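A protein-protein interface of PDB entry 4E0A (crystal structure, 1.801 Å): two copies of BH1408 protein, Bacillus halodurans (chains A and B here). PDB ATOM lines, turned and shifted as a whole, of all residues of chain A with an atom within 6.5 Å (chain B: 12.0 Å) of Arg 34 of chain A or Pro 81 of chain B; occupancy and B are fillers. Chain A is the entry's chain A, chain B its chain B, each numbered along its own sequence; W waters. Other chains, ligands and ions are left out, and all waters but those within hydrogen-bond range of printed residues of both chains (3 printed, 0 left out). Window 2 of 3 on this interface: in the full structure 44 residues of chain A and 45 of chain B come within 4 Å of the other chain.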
ATOM      1  N   HIS A  22     -16.576  25.287  28.362  1.00  0.00           N
ATOM      2  CA  HIS A  22     -16.777  25.064  26.935  1.00  0.00           C
ATOM      3  C   HIS A  22     -16.032  23.827  26.459  1.00  0.00           C
ATOM      4  O   HIS A  22     -16.598  22.989  25.755  1.00  0.00           O
ATOM      5  CB  HIS A  22     -16.354  26.245  26.075  1.00  0.00           C
ATOM      6  CG  HIS A  22     -16.790  26.091  24.654  1.00  0.00           C
ATOM      7  ND1 HIS A  22     -18.115  26.137  24.290  1.00  0.00           N
ATOM      8  CD2 HIS A  22     -16.095  25.819  23.525  1.00  0.00           C
ATOM      9  CE1 HIS A  22     -18.218  25.937  22.986  1.00  0.00           C
ATOM     10  NE2 HIS A  22     -17.008  25.745  22.498  1.00  0.00           N
ATOM     11  N   GLU A  23     -14.770  23.710  26.852  1.00  0.00           N
ATOM     12  CA  GLU A  23     -13.982  22.547  26.468  1.00  0.00           C
ATOM     13  C   GLU A  23     -14.580  21.216  26.966  1.00  0.00           C
ATOM     14  O   GLU A  23     -14.493  20.202  26.275  1.00  0.00           O
ATOM     15  CB  GLU A  23     -12.520  22.705  26.895  1.00  0.00           C
ATOM     16  CG  GLU A  23     -11.689  23.487  25.886  1.00  0.00           C
ATOM     17  CD  GLU A  23     -11.547  22.742  24.550  1.00  0.00           C
ATOM     18  OE1 GLU A  23     -11.044  21.593  24.552  1.00  0.00           O
ATOM     19  OE2 GLU A  23     -11.948  23.299  23.502  1.00  0.00           O
ATOM     20  N   VAL A  26     -17.179  20.498  24.469  1.00  0.00           N
ATOM     21  CA  VAL A  26     -16.559  20.055  23.216  1.00  0.00           C
ATOM     22  C   VAL A  26     -16.133  18.588  23.322  1.00  0.00           C
ATOM     23  O   VAL A  26     -16.332  17.800  22.400  1.00  0.00           O
ATOM     24  CB  VAL A  26     -15.356  20.934  22.827  1.00  0.00           C
ATOM     25  CG1 VAL A  26     -14.541  20.288  21.699  1.00  0.00           C
ATOM     26  CG2 VAL A  26     -15.843  22.321  22.428  1.00  0.00           C
ATOM     27  N   ARG A  29     -19.671  16.466  23.606  1.00  0.00           N
ATOM     28  CA  ARG A  29     -20.615  16.655  22.509  1.00  0.00           C
ATOM     29  C   ARG A  29     -19.968  17.502  21.415  1.00  0.00           C
ATOM     30  O   ARG A  29     -20.394  18.634  21.168  1.00  0.00           O
ATOM     31  CB  ARG A  29     -21.895  17.349  23.004  1.00  0.00           C
ATOM     32  CG  ARG A  29     -22.830  16.488  23.871  1.00  0.00           C
ATOM     33  CD  ARG A  29     -23.211  15.175  23.195  1.00  0.00           C
ATOM     34  NE  ARG A  29     -23.935  15.343  21.935  1.00  0.00           N
ATOM     35  CZ  ARG A  29     -25.262  15.317  21.812  1.00  0.00           C
ATOM     36  NH1 ARG A  29     -26.033  15.154  22.881  1.00  0.00           N
ATOM     37  NH2 ARG A  29     -25.826  15.476  20.618  1.00  0.00           N
ATOM     38  N   GLY A  30     -18.943  16.954  20.775  1.00  0.00           N
ATOM     39  CA  GLY A  30     -18.238  17.652  19.715  1.00  0.00           C
ATOM     40  C   GLY A  30     -19.083  17.834  18.467  1.00  0.00           C
ATOM     41  O   GLY A  30     -18.699  18.569  17.555  1.00  0.00           O
ATOM     42  N   ILE A  32     -22.000  19.134  18.578  1.00  0.00           N
ATOM     43  CA  ILE A  32     -22.729  20.366  18.813  1.00  0.00           C
ATOM     44  C   ILE A  32     -21.744  21.508  19.048  1.00  0.00           C
ATOM     45  O   ILE A  32     -21.893  22.596  18.488  1.00  0.00           O
ATOM     46  CB  ILE A  32     -23.704  20.213  20.028  1.00  0.00           C
ATOM     47  CG1 ILE A  32     -24.792  19.169  19.704  1.00  0.00           C
ATOM     48  CG2 ILE A  32     -24.346  21.551  20.413  1.00  0.00           C
ATOM     49  CD1 ILE A  32     -25.886  19.058  20.750  1.00  0.00           C
ATOM     50  N   PHE A  33     -20.732  21.245  19.876  1.00  0.00           N
ATOM     51  CA  PHE A  33     -19.821  22.293  20.339  1.00  0.00           C
ATOM     52  C   PHE A  33     -18.502  22.262  19.582  1.00  0.00           C
ATOM     53  O   PHE A  33     -18.006  21.205  19.208  1.00  0.00           O
ATOM     54  CB  PHE A  33     -19.593  22.171  21.857  1.00  0.00           C
ATOM     55  CG  PHE A  33     -20.847  22.360  22.664  1.00  0.00           C
ATOM     56  CD1 PHE A  33     -21.615  21.267  23.055  1.00  0.00           C
ATOM     57  CD2 PHE A  33     -21.273  23.629  23.006  1.00  0.00           C
ATOM     58  CE1 PHE A  33     -22.776  21.449  23.773  1.00  0.00           C
ATOM     59  CE2 PHE A  33     -22.437  23.819  23.735  1.00  0.00           C
ATOM     60  CZ  PHE A  33     -23.188  22.723  24.115  1.00  0.00           C
ATOM     61  N   ARG A  34     -17.936  23.438  19.364  1.00  0.00           N
ATOM     62  CA  ARG A  34     -16.735  23.570  18.559  1.00  0.00           C
ATOM     63  C   ARG A  34     -15.635  24.250  19.379  1.00  0.00           C
ATOM     64  O   ARG A  34     -15.897  25.217  20.099  1.00  0.00           O
ATOM     65  CB  ARG A  34     -17.064  24.402  17.312  1.00  0.00           C
ATOM     66  CG  ARG A  34     -15.952  24.503  16.287  1.00  0.00           C
ATOM     67  CD  ARG A  34     -16.402  25.407  15.140  1.00  0.00           C
ATOM     68  NE  ARG A  34     -15.383  25.544  14.106  1.00  0.00           N
ATOM     69  CZ  ARG A  34     -14.418  26.461  14.123  1.00  0.00           C
ATOM     70  NH1 ARG A  34     -14.326  27.324  15.136  1.00  0.00           N
ATOM     71  NH2 ARG A  34     -13.536  26.508  13.131  1.00  0.00           N
ATOM     72  N   SER A  35     -14.408  23.747  19.267  1.00  0.00           N
ATOM     73  CA  SER A  35     -13.265  24.401  19.901  1.00  0.00           C
ATOM     74  C   SER A  35     -12.988  25.731  19.234  1.00  0.00           C
ATOM     75  O   SER A  35     -13.057  25.842  18.009  1.00  0.00           O
ATOM     76  CB  SER A  35     -12.008  23.533  19.792  1.00  0.00           C
ATOM     77  OG  SER A  35     -12.060  22.445  20.694  1.00  0.00           O
ATOM     78  N   ASN A  36     -12.633  26.730  20.032  1.00  0.00           N
ATOM     79  CA  ASN A  36     -12.249  28.029  19.491  1.00  0.00           C
ATOM     80  C   ASN A  36     -11.487  28.791  20.538  1.00  0.00           C
ATOM     81  O   ASN A  36     -11.651  28.554  21.730  1.00  0.00           O
ATOM     82  CB  ASN A  36     -13.478  28.850  19.050  1.00  0.00           C
ATOM     83  CG  ASN A  36     -13.107  30.041  18.151  1.00  0.00           C
ATOM     84  OD1 ASN A  36     -12.787  29.866  16.973  1.00  0.00           O
ATOM     85  ND2 ASN A  36     -13.162  31.247  18.701  1.00  0.00           N
ATOM     86  N   GLU A  37     -10.661  29.724  20.099  1.00  0.00           N
ATOM     87  CA  GLU A  37      -9.967  30.585  21.041  1.00  0.00           C
ATOM     88  C   GLU A  37     -10.217  32.026  20.600  1.00  0.00           C
ATOM     89  O   GLU A  37      -9.783  32.420  19.514  1.00  0.00           O
ATOM     90  CB  GLU A  37      -8.463  30.274  21.021  1.00  0.00           C
ATOM     91  CG  GLU A  37      -8.111  28.792  21.187  1.00  0.00           C
ATOM     92  CD  GLU A  37      -6.605  28.550  21.143  1.00  0.00           C
ATOM     93  OE1 GLU A  37      -6.022  28.582  20.039  1.00  0.00           O
ATOM     94  OE2 GLU A  37      -6.005  28.368  22.223  1.00  0.00           O
ATOM     95  N   PRO A  38     -10.923  32.821  21.426  1.00  0.00           N
ATOM     96  CA  PRO A  38     -11.483  32.471  22.735  1.00  0.00           C
ATOM     97  C   PRO A  38     -12.817  31.777  22.565  1.00  0.00           C
ATOM     98  O   PRO A  38     -13.239  31.629  21.436  1.00  0.00           O
ATOM     99  CB  PRO A  38     -11.689  33.837  23.406  1.00  0.00           C
ATOM    100  CG  PRO A  38     -11.936  34.770  22.296  1.00  0.00           C
ATOM    101  CD  PRO A  38     -11.175  34.235  21.079  1.00  0.00           C
ATOM    102  N   THR A  39     -13.444  31.360  23.663  1.00  0.00           N
ATOM    103  CA  THR A  39     -14.762  30.733  23.615  1.00  0.00           C
ATOM    104  C   THR A  39     -15.808  31.748  24.019  1.00  0.00           C
ATOM    105  O   THR A  39     -16.990  31.541  23.801  1.00  0.00           O
ATOM    106  CB  THR A  39     -14.866  29.536  24.577  1.00  0.00           C
ATOM    107  OG1 THR A  39     -14.726  29.991  25.934  1.00  0.00           O
ATOM    108  CG2 THR A  39     -13.779  28.502  24.262  1.00  0.00           C
ATOM    109  N   THR B  77     -28.702  25.962  11.594  1.00  0.00           N
ATOM    110  CA  THR B  77     -27.934  26.926  12.384  1.00  0.00           C
ATOM    111  C   THR B  77     -26.670  27.278  11.625  1.00  0.00           C
ATOM    112  O   THR B  77     -26.039  26.398  11.046  1.00  0.00           O
ATOM    113  CB  THR B  77     -27.478  26.332  13.730  1.00  0.00           C
ATOM    114  OG1 THR B  77     -26.430  25.379  13.497  1.00  0.00           O
ATOM    115  CG2 THR B  77     -28.642  25.668  14.460  1.00  0.00           C
ATOM    116  N   PRO B  78     -26.275  28.562  11.639  1.00  0.00           N
ATOM    117  CA  PRO B  78     -25.100  28.966  10.865  1.00  0.00           C
ATOM    118  C   PRO B  78     -23.830  28.571  11.604  1.00  0.00           C
ATOM    119  O   PRO B  78     -23.890  28.341  12.811  1.00  0.00           O
ATOM    120  CB  PRO B  78     -25.218  30.490  10.847  1.00  0.00           C
ATOM    121  CG  PRO B  78     -25.856  30.809  12.169  1.00  0.00           C
ATOM    122  CD  PRO B  78     -26.795  29.663  12.474  1.00  0.00           C
ATOM    123  N   LEU B  79     -22.702  28.505  10.905  1.00  0.00           N
ATOM    124  CA  LEU B  79     -21.437  28.247  11.578  1.00  0.00           C
ATOM    125  C   LEU B  79     -21.127  29.384  12.549  1.00  0.00           C
ATOM    126  O   LEU B  79     -21.301  30.550  12.217  1.00  0.00           O
ATOM    127  CB  LEU B  79     -20.301  28.075  10.570  1.00  0.00           C
ATOM    128  CG  LEU B  79     -18.922  27.852  11.192  1.00  0.00           C
ATOM    129  CD1 LEU B  79     -18.939  26.666  12.160  1.00  0.00           C
ATOM    130  CD2 LEU B  79     -17.870  27.664  10.112  1.00  0.00           C
ATOM    131  N   LEU B  80     -20.706  29.031  13.760  1.00  0.00           N
ATOM    132  CA  LEU B  80     -20.279  30.014  14.752  1.00  0.00           C
ATOM    133  C   LEU B  80     -18.916  29.580  15.273  1.00  0.00           C
ATOM    134  O   LEU B  80     -18.537  28.427  15.111  1.00  0.00           O
ATOM    135  CB  LEU B  80     -21.273  30.078  15.911  1.00  0.00           C
ATOM    136  CG  LEU B  80     -22.643  30.671  15.599  1.00  0.00           C
ATOM    137  CD1 LEU B  80     -23.586  30.405  16.757  1.00  0.00           C
ATOM    138  CD2 LEU B  80     -22.521  32.173  15.325  1.00  0.00           C
ATOM    139  N   PRO B  81     -18.171  30.507  15.892  1.00  0.00           N
ATOM    140  CA  PRO B  81     -16.852  30.111  16.389  1.00  0.00           C
ATOM    141  C   PRO B  81     -16.943  28.952  17.378  1.00  0.00           C
ATOM    142  O   PRO B  81     -16.097  28.064  17.351  1.00  0.00           O
ATOM    143  CB  PRO B  81     -16.359  31.371  17.094  1.00  0.00           C
ATOM    144  CG  PRO B  81     -17.031  32.493  16.339  1.00  0.00           C
ATOM    145  CD  PRO B  81     -18.402  31.958  16.028  1.00  0.00           C
ATOM    146  N   THR B  82     -17.964  28.947  18.224  1.00  0.00           N
ATOM    147  CA  THR B  82     -18.013  27.950  19.281  1.00  0.00           C
ATOM    148  C   THR B  82     -19.107  26.907  19.096  1.00  0.00           C
ATOM    149  O   THR B  82     -19.281  26.044  19.959  1.00  0.00           O
ATOM    150  CB  THR B  82     -18.161  28.608  20.679  1.00  0.00           C
ATOM    151  OG1 THR B  82     -19.427  29.277  20.768  1.00  0.00           O
ATOM    152  CG2 THR B  82     -17.041  29.599  20.922  1.00  0.00           C
ATOM    153  N   MET B  83     -19.849  26.969  17.987  1.00  0.00           N
ATOM    154  CA  MET B  83     -20.881  25.950  17.725  1.00  0.00           C
ATOM    155  C   MET B  83     -20.786  25.401  16.304  1.00  0.00           C
ATOM    156  O   MET B  83     -20.604  26.156  15.340  1.00  0.00           O
ATOM    157  CB  MET B  83     -22.306  26.481  17.958  1.00  0.00           C
ATOM    158  CG  MET B  83     -22.552  27.138  19.308  1.00  0.00           C
ATOM    159  SD  MET B  83     -22.544  25.872  20.773  1.00  0.00           S
ATOM    160  CE  MET B  83     -24.369  25.197  20.616  1.00  0.00           C
ATOM    161  N   GLN B  84     -20.911  24.083  16.182  1.00  0.00           N
ATOM    162  CA  GLN B  84     -20.939  23.451  14.874  1.00  0.00           C
ATOM    163  C   GLN B  84     -22.155  23.928  14.103  1.00  0.00           C
ATOM    164  O   GLN B  84     -23.200  24.184  14.688  1.00  0.00           O
ATOM    165  CB  GLN B  84     -20.995  21.933  15.004  1.00  0.00           C
ATOM    166  CG  GLN B  84     -19.884  21.334  15.850  1.00  0.00           C
ATOM    167  CD  GLN B  84     -18.518  21.453  15.205  1.00  0.00           C
ATOM    168  OE1 GLN B  84     -18.357  22.079  14.153  1.00  0.00           O
ATOM    169  NE2 GLN B  84     -17.523  20.846  15.832  1.00  0.00           N
ATOM    170  N   GLN B  85     -21.999  24.063  12.793  1.00  0.00           N
ATOM    171  CA  GLN B  85     -23.135  24.249  11.914  1.00  0.00           C
ATOM    172  C   GLN B  85     -23.991  22.992  12.039  1.00  0.00           C
ATOM    173  O   GLN B  85     -23.471  21.883  12.080  1.00  0.00           O
ATOM    174  CB  GLN B  85     -22.648  24.430  10.479  1.00  0.00           C
ATOM    175  CG  GLN B  85     -23.748  24.648   9.455  1.00  0.00           C
ATOM    176  CD  GLN B  85     -23.189  24.966   8.079  1.00  0.00           C
ATOM    177  OE1 GLN B  85     -22.414  25.906   7.917  1.00  0.00           O
ATOM    178  NE2 GLN B  85     -23.570  24.172   7.085  1.00  0.00           N
ATOM    179  N   ARG B  86     -25.301  23.152  12.124  1.00  0.00           N
ATOM    180  CA  ARG B  86     -26.135  21.984  12.348  1.00  0.00           C
ATOM    181  C   ARG B  86     -27.449  22.069  11.594  1.00  0.00           C
ATOM    182  O   ARG B  86     -28.087  23.120  11.561  1.00  0.00           O
ATOM    183  CB  ARG B  86     -26.383  21.801  13.845  1.00  0.00           C
ATOM    184  CG  ARG B  86     -26.797  20.401  14.218  1.00  0.00           C
ATOM    185  CD  ARG B  86     -26.065  19.929  15.466  1.00  0.00           C
ATOM    186  NE  ARG B  86     -26.682  18.720  15.996  1.00  0.00           N
ATOM    187  CZ  ARG B  86     -27.809  18.731  16.695  1.00  0.00           C
ATOM    188  NH1 ARG B  86     -28.421  19.883  16.940  1.00  0.00           N
ATOM    189  NH2 ARG B  86     -28.320  17.603  17.155  1.00  0.00           N
HETATM  190  O   HOH W   1     -24.100  23.276  17.155  1.00  0.00           O
HETATM  191  O   HOH W   2     -15.667  19.324  18.053  1.00  0.00           O
HETATM  192  O   HOH W   3     -16.144  23.120  12.743  1.00  0.00           O
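The side-chain amide nitrogen (NE2) of Gln 84 of chain B lies within hydrogen-bond range of the backbone carbonyl oxygen (O) of Phe 33 of chain A. The backbone carbonyl oxygen (O) of Pro 81 of chain B lies within hydrogen-bond range of the guanidinium group (NH1) of Arg 34 of chain A, at 2.9 Å. The side-chain amide nitrogen (NE2) of Gln 84 of chain B is in hydrogen-bond range of the backbone carbonyl oxygen (O) of Gly 30 of chain A, at 3.1 Å. A ring nitrogen (NE2) of His 22 of chain A sits close to the backbone carbonyl oxygen (O) of Thr 82 of chain B (3.4 Å). The backbone carbonyl oxygen of Thr 82 of chain B is in hydrogen-bond range of the backbone NH of Arg 34 of chain A (3.0 Å). The backbone carbonyl oxygen (O) of Ile 32 of chain A is in hydrogen-bond range of the backbone NH (N) of Gln 84 of chain B (2.9 Å).
NE2 of His 22 of chain A is in hydrogen-bond range of O of Arg 34 of chain A. The side-chain amide nitrogen (ND2) of Asn 36 of chain A is in hydrogen-bond range of the backbone carbonyl oxygen (O) of Pro 38 of chain A (2.8 Å). The side-chain hydroxyl (OG) of Ser 35 of chain A lies within hydrogen-bond range of the side-chain carboxylate (OE2) of Glu 23 of chain A, at 2.9 Å. NH1 of Arg 34 of chain A sits at hydrogen-bond distance from OD1 of Asn 36 of chain A (3.5 Å).
Among the printed residues, pairs that only touch across the chains: Ile 32 of chain A with Met 83 of chain B, Phe 33 of chain A with Thr 82 of chain B, Phe 33 of chain A with Met 83 of chain B, Arg 34 of chain A with Leu 80 of chain B, Arg 34 of chain A with Met 83 of chain B, Arg 34 of chain A with Gln 84 of chain B, Ser 35 of chain A with Pro 81 of chain B, Asn 36 of chain A with Pro 81 of chain B and Thr 39 of chain A with Thr 82 of chain B.
Of the printed residues of chain B, His 22 of chain A touches Thr 82 (3.2 Å). Gly 30 of chain A touches one residue of chain B. Arg 34 of chain A touches just these residues of chain B: Leu 80 (3.7 Å), Pro 81 (2.9 Å), Thr 82 (3.0 Å), Met 83 (3.8 Å) and Gln 84 (3.9 Å). Of the printed residues of chain B, Asn 36 of chain A touches Pro 81. Of the printed residues of chain B, Thr 39 of chain A touches Thr 82 (3.5 Å). Printed residues of chain A within 4 Å of Leu 80 of chain B: Arg 34 (3.7 Å). Pro 81 of chain B touches just these residues of chain A: Arg 34, Ser 35 and Asn 36. Printed residues of chain A within 4 Å of Thr 82 of chain B: His 22, Phe 33, Arg 34 and Thr 39. Printed residues of chain A within 4 Å of Met 83 of chain B: Ile 32 (3.6 Å), Phe 33 (3.4 Å) and Arg 34 (3.8 Å). Of the printed residues of chain A, Gln 84 of chain B touches Gly 30, Ile 32, Phe 33 and Arg 34. Gln 85 of chain B touches none of the printed residues of chain A. The nearest residue of chain A that does not touch Pro 81 of chain B is Pro 38 of chain A (5.4 Å). The nearest printed residue of chain A that does not touch Met 83 of chain B is His 22 of chain A (4.9 Å).
Of the 13 printed residues of chain A, 8 touch a printed residue of chain B. Hydrophobic or aromatic side chains of chain A that line the printed part of chain B: His 22, Ile 32 and Phe 33. Printed residues of chain B that touch a printed residue of chain A: Leu 80, Pro 81, Thr 82, Met 83 and Gln 84. Hydrophobic or aromatic side chains of chain B that line the printed part of chain A: Pro 81 and Met 83. Among the printed residues, no Asp or Glu carboxylate lies within 4 Å of a Lys or Arg side-chain nitrogen of the other chain.
No position is printed for both chains. Of the 15 pairs that touch across the chains among the printed residues, none has its exchanged pair printed and touching as well.
Water W1 lies within hydrogen-bond range of the backbone carbonyl oxygen of Ile 32 of chain A (2.7 Å) and the backbone carbonyl oxygen of Gln 84 of chain B (2.8 Å). Water W3 lies within hydrogen-bond range of OE1 of Gln 84 of chain B and NE of Arg 34 of chain A. Water W2 lies within hydrogen-bond range of O of Gly 30 of chain A, O of Phe 33 of chain A and NE2 of Gln 84 of chain B.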
